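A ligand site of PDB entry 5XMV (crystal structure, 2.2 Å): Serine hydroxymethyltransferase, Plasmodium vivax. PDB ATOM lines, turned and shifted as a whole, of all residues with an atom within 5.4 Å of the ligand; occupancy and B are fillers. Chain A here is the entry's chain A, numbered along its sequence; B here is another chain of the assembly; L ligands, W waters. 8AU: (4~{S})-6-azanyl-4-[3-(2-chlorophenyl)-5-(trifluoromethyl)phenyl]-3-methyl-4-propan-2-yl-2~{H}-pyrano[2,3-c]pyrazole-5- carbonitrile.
The side-chain amino group (NZ) of Lys 355 lies close to a fluorine (F32) of the ligand.
The backbone carbonyl oxygen (O) of Cys 364 sits close to a fluorine (F30) of the ligand (3.2 Å).
Merely in contact with the ligand: Gly 127, His 129, Leu 130, Asn 354, Pro 367, Arg 371, Tyr 63 of chain B, Tyr 64 of chain B and Phe 266 of chain B.
Hydrophobic or aromatic side chains that line the ligand: Leu 124, His 129, Leu 130, Pro 367, Tyr 63 of chain B, Tyr 64 of chain B and Phe 266 of chain B.
Along chain A the residues within 4 Å of the ligand span positions 124 to 371.
ND2 of Asn 356 is in hydrogen-bond range of N9 of the ligand (3.5 Å).
The side-chain hydroxyl of Thr 183 is in hydrogen-bond range of an oxygen (O1) of the ligand.
The backbone carbonyl oxygen (O) of Gly 128 is in hydrogen-bond range of a nitrogen (N7) of the ligand (2.7 Å).
The side-chain hydroxyl (OG1) of Thr 357 is in hydrogen-bond range of a nitrogen (N9) of the ligand (3.3 Å).
OE2 of Glu 56 of chain B sits at hydrogen-bond distance from N11 of the ligand (2.9 Å).
The backbone carbonyl oxygen (O) of Leu 124 sits at hydrogen-bond distance from a nitrogen (N7) of the ligand, 3.1 Å away.
O of Thr 183 sits at hydrogen-bond distance from NH1 of Arg 371.
N of Thr 183 sits at hydrogen-bond distance from O of Gly 127 (2.7 Å).
O of Gly 127 lies within hydrogen-bond range of N of Ser 184 (3.3 Å).
O of Glu 56 of chain B sits at hydrogen-bond distance from N of Tyr 63 of chain B (3.1 Å).
The backbone carbonyl oxygen (O) of Cys 125 is in hydrogen-bond range of the side-chain hydroxyl (OG1) of Thr 357 (2.7 Å).
SG of Cys 364 lies within hydrogen-bond range of SG of Cys 125.
The backbone carbonyl oxygen (O) of Tyr 63 of chain B lies within hydrogen-bond range of the side-chain amino group (NZ) of Lys 355 (3.5 Å).
The side-chain amide oxygen (OD1) of Asn 356 lies within hydrogen-bond range of the side-chain hydroxyl (OG) of Ser 184, at 3.3 Å.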
ATOM      1  N   LEU A 124       9.102  27.415  15.252  1.00  0.00           N
ATOM      2  CA  LEU A 124       9.016  26.311  16.230  1.00  0.00           C
ATOM      3  C   LEU A 124       9.356  26.794  17.636  1.00  0.00           C
ATOM      4  O   LEU A 124       8.598  26.555  18.574  1.00  0.00           O
ATOM      5  CB  LEU A 124       9.963  25.163  15.842  1.00  0.00           C
ATOM      6  CG  LEU A 124      10.082  23.947  16.784  1.00  0.00           C
ATOM      7  CD1 LEU A 124       9.064  22.861  16.465  1.00  0.00           C
ATOM      8  CD2 LEU A 124      11.480  23.366  16.717  1.00  0.00           C
ATOM      9  N   CYS A 125      10.511  27.451  17.748  1.00  0.00           N
ATOM     10  CA  CYS A 125      10.970  28.145  18.969  1.00  0.00           C
ATOM     11  C   CYS A 125       9.986  29.152  19.591  1.00  0.00           C
ATOM     12  O   CYS A 125      10.122  29.473  20.753  1.00  0.00           O
ATOM     13  CB  CYS A 125      12.325  28.855  18.720  1.00  0.00           C
ATOM     14  SG  CYS A 125      13.656  27.788  18.052  1.00  0.00           S
ATOM     15  N   GLY A 127       6.566  28.511  19.396  1.00  0.00           N
ATOM     16  CA  GLY A 127       5.337  27.754  19.666  1.00  0.00           C
ATOM     17  C   GLY A 127       4.615  27.191  18.453  1.00  0.00           C
ATOM     18  O   GLY A 127       3.581  26.558  18.619  1.00  0.00           O
ATOM     19  N   GLY A 128       5.166  27.390  17.247  1.00  0.00           N
ATOM     20  CA  GLY A 128       4.646  26.725  16.046  1.00  0.00           C
ATOM     21  C   GLY A 128       5.018  25.251  15.979  1.00  0.00           C
ATOM     22  O   GLY A 128       5.901  24.779  16.713  1.00  0.00           O
ATOM     23  N   HIS A 129       4.306  24.490  15.139  1.00  0.00           N
ATOM     24  CA  HIS A 129       4.658  23.111  14.877  1.00  0.00           C
ATOM     25  C   HIS A 129       5.742  22.971  13.832  1.00  0.00           C
ATOM     26  O   HIS A 129       5.982  23.856  13.048  1.00  0.00           O
ATOM     27  CB  HIS A 129       3.430  22.281  14.490  1.00  0.00           C
ATOM     28  CG  HIS A 129       3.651  20.803  14.614  1.00  0.00           C
ATOM     29  ND1 HIS A 129       3.649  19.956  13.530  1.00  0.00           N
ATOM     30  CD2 HIS A 129       3.947  20.029  15.689  1.00  0.00           C
ATOM     31  CE1 HIS A 129       3.913  18.723  13.930  1.00  0.00           C
ATOM     32  NE2 HIS A 129       4.082  18.741  15.241  1.00  0.00           N
ATOM     33  N   LEU A 130       6.413  21.819  13.878  1.00  0.00           N
ATOM     34  CA  LEU A 130       7.410  21.412  12.873  1.00  0.00           C
ATOM     35  C   LEU A 130       6.852  21.493  11.443  1.00  0.00           C
ATOM     36  O   LEU A 130       7.552  21.941  10.556  1.00  0.00           O
ATOM     37  CB  LEU A 130       7.873  19.977  13.129  1.00  0.00           C
ATOM     38  CG  LEU A 130       8.573  19.721  14.463  1.00  0.00           C
ATOM     39  CD1 LEU A 130       8.401  18.265  14.864  1.00  0.00           C
ATOM     40  CD2 LEU A 130      10.056  20.093  14.360  1.00  0.00           C
ATOM     41  N   PHE A 134       9.013  24.529   9.511  1.00  0.00           N
ATOM     42  CA  PHE A 134      10.222  24.696  10.290  1.00  0.00           C
ATOM     43  C   PHE A 134      11.501  24.348   9.552  1.00  0.00           C
ATOM     44  O   PHE A 134      11.621  23.253   8.995  1.00  0.00           O
ATOM     45  CB  PHE A 134      10.209  23.904  11.587  1.00  0.00           C
ATOM     46  CG  PHE A 134      11.367  24.225  12.457  1.00  0.00           C
ATOM     47  CD1 PHE A 134      11.559  25.522  12.918  1.00  0.00           C
ATOM     48  CD2 PHE A 134      12.340  23.273  12.711  1.00  0.00           C
ATOM     49  CE1 PHE A 134      12.673  25.855  13.666  1.00  0.00           C
ATOM     50  CE2 PHE A 134      13.463  23.609  13.455  1.00  0.00           C
ATOM     51  CZ  PHE A 134      13.622  24.900  13.941  1.00  0.00           C
ATOM     52  N   VAL A 141      14.630  21.255   8.316  1.00  0.00           N
ATOM     53  CA  VAL A 141      14.324  20.220   9.318  1.00  0.00           C
ATOM     54  C   VAL A 141      12.995  19.494   8.979  1.00  0.00           C
ATOM     55  O   VAL A 141      12.911  18.260   9.029  1.00  0.00           O
ATOM     56  CB  VAL A 141      14.278  20.851  10.741  1.00  0.00           C
ATOM     57  CG1 VAL A 141      13.705  19.920  11.794  1.00  0.00           C
ATOM     58  CG2 VAL A 141      15.671  21.329  11.170  1.00  0.00           C
ATOM     59  N   THR A 183       1.545  24.785  18.776  1.00  0.00           N
ATOM     60  CA  THR A 183       1.836  23.624  19.631  1.00  0.00           C
ATOM     61  C   THR A 183       1.972  24.015  21.079  1.00  0.00           C
ATOM     62  O   THR A 183       1.556  23.265  21.931  1.00  0.00           O
ATOM     63  CB  THR A 183       2.997  22.710  19.168  1.00  0.00           C
ATOM     64  OG1 THR A 183       4.135  22.790  20.043  1.00  0.00           O
ATOM     65  CG2 THR A 183       3.384  22.980  17.792  1.00  0.00           C
ATOM     66  N   SER A 184       2.486  25.211  21.368  1.00  0.00           N
ATOM     67  CA  SER A 184       2.572  25.680  22.756  1.00  0.00           C
ATOM     68  C   SER A 184       2.381  27.177  22.867  1.00  0.00           C
ATOM     69  O   SER A 184       3.304  27.916  23.149  1.00  0.00           O
ATOM     70  CB  SER A 184       3.897  25.232  23.391  1.00  0.00           C
ATOM     71  OG  SER A 184       4.994  25.772  22.698  1.00  0.00           O
ATOM     72  N   ASN A 354       7.406  18.664  29.529  1.00  0.00           N
ATOM     73  CA  ASN A 354       8.441  18.813  28.525  1.00  0.00           C
ATOM     74  C   ASN A 354       9.077  20.153  28.538  1.00  0.00           C
ATOM     75  O   ASN A 354       8.465  21.152  28.901  1.00  0.00           O
ATOM     76  CB  ASN A 354       7.942  18.463  27.101  1.00  0.00           C
ATOM     77  CG  ASN A 354       6.860  19.399  26.601  1.00  0.00           C
ATOM     78  OD1 ASN A 354       5.691  19.117  26.781  1.00  0.00           O
ATOM     79  ND2 ASN A 354       7.241  20.504  26.007  1.00  0.00           N
ATOM     80  N   LYS A 355      10.336  20.159  28.130  1.00  0.00           N
ATOM     81  CA  LYS A 355      11.082  21.375  27.957  1.00  0.00           C
ATOM     82  C   LYS A 355      10.496  22.188  26.816  1.00  0.00           C
ATOM     83  O   LYS A 355       9.934  21.638  25.831  1.00  0.00           O
ATOM     84  CB  LYS A 355      12.589  21.094  27.758  1.00  0.00           C
ATOM     85  CG  LYS A 355      12.964  20.148  26.608  1.00  0.00           C
ATOM     86  CD  LYS A 355      14.484  20.162  26.365  1.00  0.00           C
ATOM     87  CE  LYS A 355      15.078  18.758  26.318  1.00  0.00           C
ATOM     88  NZ  LYS A 355      14.791  18.031  25.055  1.00  0.00           N
ATOM     89  N   ASN A 356      10.600  23.495  26.933  1.00  0.00           N
ATOM     90  CA  ASN A 356       9.935  24.374  25.990  1.00  0.00           C
ATOM     91  C   ASN A 356      10.650  25.706  25.918  1.00  0.00           C
ATOM     92  O   ASN A 356      11.072  26.263  26.939  1.00  0.00           O
ATOM     93  CB  ASN A 356       8.446  24.539  26.363  1.00  0.00           C
ATOM     94  CG  ASN A 356       7.576  24.799  25.142  1.00  0.00           C
ATOM     95  OD1 ASN A 356       6.868  23.901  24.642  1.00  0.00           O
ATOM     96  ND2 ASN A 356       7.666  26.004  24.619  1.00  0.00           N
ATOM     97  N   THR A 357      10.786  26.217  24.709  1.00  0.00           N
ATOM     98  CA  THR A 357      11.390  27.525  24.472  1.00  0.00           C
ATOM     99  C   THR A 357      10.538  28.660  25.035  1.00  0.00           C
ATOM    100  O   THR A 357       9.366  28.455  25.338  1.00  0.00           O
ATOM    101  CB  THR A 357      11.612  27.741  22.968  1.00  0.00           C
ATOM    102  OG1 THR A 357      10.490  27.200  22.247  1.00  0.00           O
ATOM    103  CG2 THR A 357      12.896  27.038  22.492  1.00  0.00           C
ATOM    104  N   CYS A 364      17.344  26.736  20.233  1.00  0.00           N
ATOM    105  CA  CYS A 364      16.686  25.543  20.803  1.00  0.00           C
ATOM    106  C   CYS A 364      17.590  24.684  21.714  1.00  0.00           C
ATOM    107  O   CYS A 364      17.087  23.770  22.384  1.00  0.00           O
ATOM    108  CB  CYS A 364      16.088  24.644  19.705  1.00  0.00           C
ATOM    109  SG  CYS A 364      14.289  24.729  19.604  1.00  0.00           S
ATOM    110  N   VAL A 365      18.894  24.932  21.699  1.00  0.00           N
ATOM    111  CA  VAL A 365      19.805  24.425  22.737  1.00  0.00           C
ATOM    112  C   VAL A 365      19.539  25.249  24.002  1.00  0.00           C
ATOM    113  O   VAL A 365      19.571  26.484  23.969  1.00  0.00           O
ATOM    114  CB  VAL A 365      21.289  24.534  22.314  1.00  0.00           C
ATOM    115  CG1 VAL A 365      22.217  24.136  23.470  1.00  0.00           C
ATOM    116  CG2 VAL A 365      21.569  23.683  21.077  1.00  0.00           C
ATOM    117  N   PRO A 367      16.518  25.445  26.134  1.00  0.00           N
ATOM    118  CA  PRO A 367      15.258  26.180  26.288  1.00  0.00           C
ATOM    119  C   PRO A 367      15.029  26.500  27.762  1.00  0.00           C
ATOM    120  O   PRO A 367      15.296  25.659  28.635  1.00  0.00           O
ATOM    121  CB  PRO A 367      14.210  25.166  25.828  1.00  0.00           C
ATOM    122  CG  PRO A 367      14.818  23.830  26.140  1.00  0.00           C
ATOM    123  CD  PRO A 367      16.272  24.017  25.812  1.00  0.00           C
ATOM    124  N   ARG A 371       6.662  23.327  29.389  1.00  0.00           N
ATOM    125  CA  ARG A 371       5.289  23.416  29.097  1.00  0.00           C
ATOM    126  C   ARG A 371       4.558  22.364  29.888  1.00  0.00           C
ATOM    127  O   ARG A 371       5.008  21.186  29.926  1.00  0.00           O
ATOM    128  CB  ARG A 371       5.092  23.203  27.601  1.00  0.00           C
ATOM    129  CG  ARG A 371       3.647  23.276  27.132  1.00  0.00           C
ATOM    130  CD  ARG A 371       3.578  22.794  25.697  1.00  0.00           C
ATOM    131  NE  ARG A 371       3.659  21.346  25.620  1.00  0.00           N
ATOM    132  CZ  ARG A 371       3.418  20.611  24.532  1.00  0.00           C
ATOM    133  NH1 ARG A 371       3.063  21.191  23.376  1.00  0.00           N
ATOM    134  NH2 ARG A 371       3.535  19.280  24.617  1.00  0.00           N
ATOM    135  N   GLU B  56       8.213  11.308  20.608  1.00  0.00           N
ATOM    136  CA  GLU B  56       8.970  11.850  19.488  1.00  0.00           C
ATOM    137  C   GLU B  56      10.457  11.680  19.637  1.00  0.00           C
ATOM    138  O   GLU B  56      11.009  11.919  20.682  1.00  0.00           O
ATOM    139  CB  GLU B  56       8.658  13.330  19.329  1.00  0.00           C
ATOM    140  CG  GLU B  56       7.326  13.582  18.665  1.00  0.00           C
ATOM    141  CD  GLU B  56       6.909  15.023  18.757  1.00  0.00           C
ATOM    142  OE1 GLU B  56       6.588  15.465  19.872  1.00  0.00           O
ATOM    143  OE2 GLU B  56       6.950  15.732  17.728  1.00  0.00           O
ATOM    144  N   TYR B  63      12.670  13.249  22.877  1.00  0.00           N
ATOM    145  CA  TYR B  63      12.463  14.647  23.249  1.00  0.00           C
ATOM    146  C   TYR B  63      11.939  14.725  24.656  1.00  0.00           C
ATOM    147  O   TYR B  63      12.303  15.644  25.385  1.00  0.00           O
ATOM    148  CB  TYR B  63      11.604  15.457  22.224  1.00  0.00           C
ATOM    149  CG  TYR B  63      12.514  16.028  21.147  1.00  0.00           C
ATOM    150  CD1 TYR B  63      12.906  15.269  20.061  1.00  0.00           C
ATOM    151  CD2 TYR B  63      13.070  17.290  21.291  1.00  0.00           C
ATOM    152  CE1 TYR B  63      13.801  15.761  19.122  1.00  0.00           C
ATOM    153  CE2 TYR B  63      13.963  17.804  20.344  1.00  0.00           C
ATOM    154  CZ  TYR B  63      14.321  17.025  19.268  1.00  0.00           C
ATOM    155  OH  TYR B  63      15.187  17.508  18.313  1.00  0.00           O
ATOM    156  N   TYR B  64      11.094  13.775  25.054  1.00  0.00           N
ATOM    157  CA  TYR B  64      10.616  13.706  26.434  1.00  0.00           C
ATOM    158  C   TYR B  64      11.221  12.544  27.200  1.00  0.00           C
ATOM    159  O   TYR B  64      11.790  11.651  26.605  1.00  0.00           O
ATOM    160  CB  TYR B  64       9.110  13.525  26.503  1.00  0.00           C
ATOM    161  CG  TYR B  64       8.338  14.455  25.649  1.00  0.00           C
ATOM    162  CD1 TYR B  64       8.848  15.705  25.280  1.00  0.00           C
ATOM    163  CD2 TYR B  64       7.066  14.112  25.214  1.00  0.00           C
ATOM    164  CE1 TYR B  64       8.105  16.556  24.488  1.00  0.00           C
ATOM    165  CE2 TYR B  64       6.315  14.960  24.426  1.00  0.00           C
ATOM    166  CZ  TYR B  64       6.832  16.174  24.065  1.00  0.00           C
ATOM    167  OH  TYR B  64       6.050  16.981  23.280  1.00  0.00           O
ATOM    168  N   PHE B 266      11.487  10.986  11.142  1.00  0.00           N
ATOM    169  CA  PHE B 266      11.276  12.085  12.105  1.00  0.00           C
ATOM    170  C   PHE B 266      12.566  12.915  12.242  1.00  0.00           C
ATOM    171  O   PHE B 266      13.605  12.333  12.428  1.00  0.00           O
ATOM    172  CB  PHE B 266      10.874  11.553  13.477  1.00  0.00           C
ATOM    173  CG  PHE B 266      10.799  12.616  14.535  1.00  0.00           C
ATOM    174  CD1 PHE B 266       9.636  13.350  14.737  1.00  0.00           C
ATOM    175  CD2 PHE B 266      11.913  12.905  15.342  1.00  0.00           C
ATOM    176  CE1 PHE B 266       9.563  14.340  15.697  1.00  0.00           C
ATOM    177  CE2 PHE B 266      11.846  13.889  16.308  1.00  0.00           C
ATOM    178  CZ  PHE B 266      10.676  14.608  16.483  1.00  0.00           C
ATOM    179  N   PRO B 267      12.489  14.249  12.192  1.00  0.00           N
ATOM    180  CA  PRO B 267      11.251  15.008  12.176  1.00  0.00           C
ATOM    181  C   PRO B 267      10.851  15.528  10.770  1.00  0.00           C
ATOM    182  O   PRO B 267       9.990  16.405  10.695  1.00  0.00           O
ATOM    183  CB  PRO B 267      11.614  16.188  13.083  1.00  0.00           C
ATOM    184  CG  PRO B 267      13.004  16.507  12.642  1.00  0.00           C
ATOM    185  CD  PRO B 267      13.643  15.166  12.340  1.00  0.00           C
HETATM  186  C4  8AU L   1       8.501  21.133  20.679  1.00  0.00           C
HETATM  187  C6  8AU L   1       6.954  20.667  18.622  1.00  0.00           C
HETATM  188  C8  8AU L   1       8.573  23.491  21.188  1.00  0.00           C
HETATM  189  C15 8AU L   1       8.427  19.445  22.682  1.00  0.00           C
HETATM  190  C17 8AU L   1      10.840  21.423  21.702  1.00  0.00           C
HETATM  191  C22 8AU L   1      12.839  20.266  18.092  1.00  0.00           C
HETATM  192  C2  8AU L   1       7.193  22.945  19.481  1.00  0.00           C
HETATM  193  C3  8AU L   1       8.087  22.600  20.429  1.00  0.00           C
HETATM  194  N9  8AU L   1       9.030  24.318  21.887  1.00  0.00           N
HETATM  195  C14 8AU L   1       7.902  20.749  22.065  1.00  0.00           C
HETATM  196  C18 8AU L   1      12.246  21.394  21.644  1.00  0.00           C
HETATM  197 CL3  8AU L   1      11.269  17.906  17.855  1.00  0.00          CL
HETATM  198  C25 8AU L   1      12.547  19.030  17.321  1.00  0.00           C
HETATM  199  C26 8AU L   1      13.258  18.721  16.187  1.00  0.00           C
HETATM  200  C27 8AU L   1      14.263  19.581  15.750  1.00  0.00           C
HETATM  201  C28 8AU L   1      14.562  20.743  16.452  1.00  0.00           C
HETATM  202  C29 8AU L   1      13.857  21.089  17.604  1.00  0.00           C
HETATM  203  C20 8AU L   1      12.104  20.654  19.334  1.00  0.00           C
HETATM  204  C19 8AU L   1      12.853  21.008  20.456  1.00  0.00           C
HETATM  205  C23 8AU L   1      13.125  21.751  22.836  1.00  0.00           C
HETATM  206  F32 8AU L   1      13.657  20.641  23.340  1.00  0.00           F
HETATM  207  F31 8AU L   1      12.452  22.377  23.785  1.00  0.00           F
HETATM  208  F30 8AU L   1      14.146  22.522  22.429  1.00  0.00           F
HETATM  209  C21 8AU L   1      10.703  20.706  19.397  1.00  0.00           C
HETATM  210  C16 8AU L   1      10.034  21.070  20.585  1.00  0.00           C
HETATM  211  C24 8AU L   1       6.369  20.756  22.116  1.00  0.00           C
HETATM  212  N7  8AU L   1       6.775  24.183  19.250  1.00  0.00           N
HETATM  213  C5  8AU L   1       7.899  20.218  19.655  1.00  0.00           C
HETATM  214  C10 8AU L   1       8.021  18.772  19.313  1.00  0.00           C
HETATM  215  C13 8AU L   1       8.858  17.710  19.981  1.00  0.00           C
HETATM  216  N11 8AU L   1       7.217  18.566  18.246  1.00  0.00           N
HETATM  217  N12 8AU L   1       6.544  19.713  17.776  1.00  0.00           N
HETATM  218  O1  8AU L   1       6.591  21.963  18.612  1.00  0.00           O
HETATM  219  O   HOH W   1      16.462  19.653  18.828  1.00  0.00           O
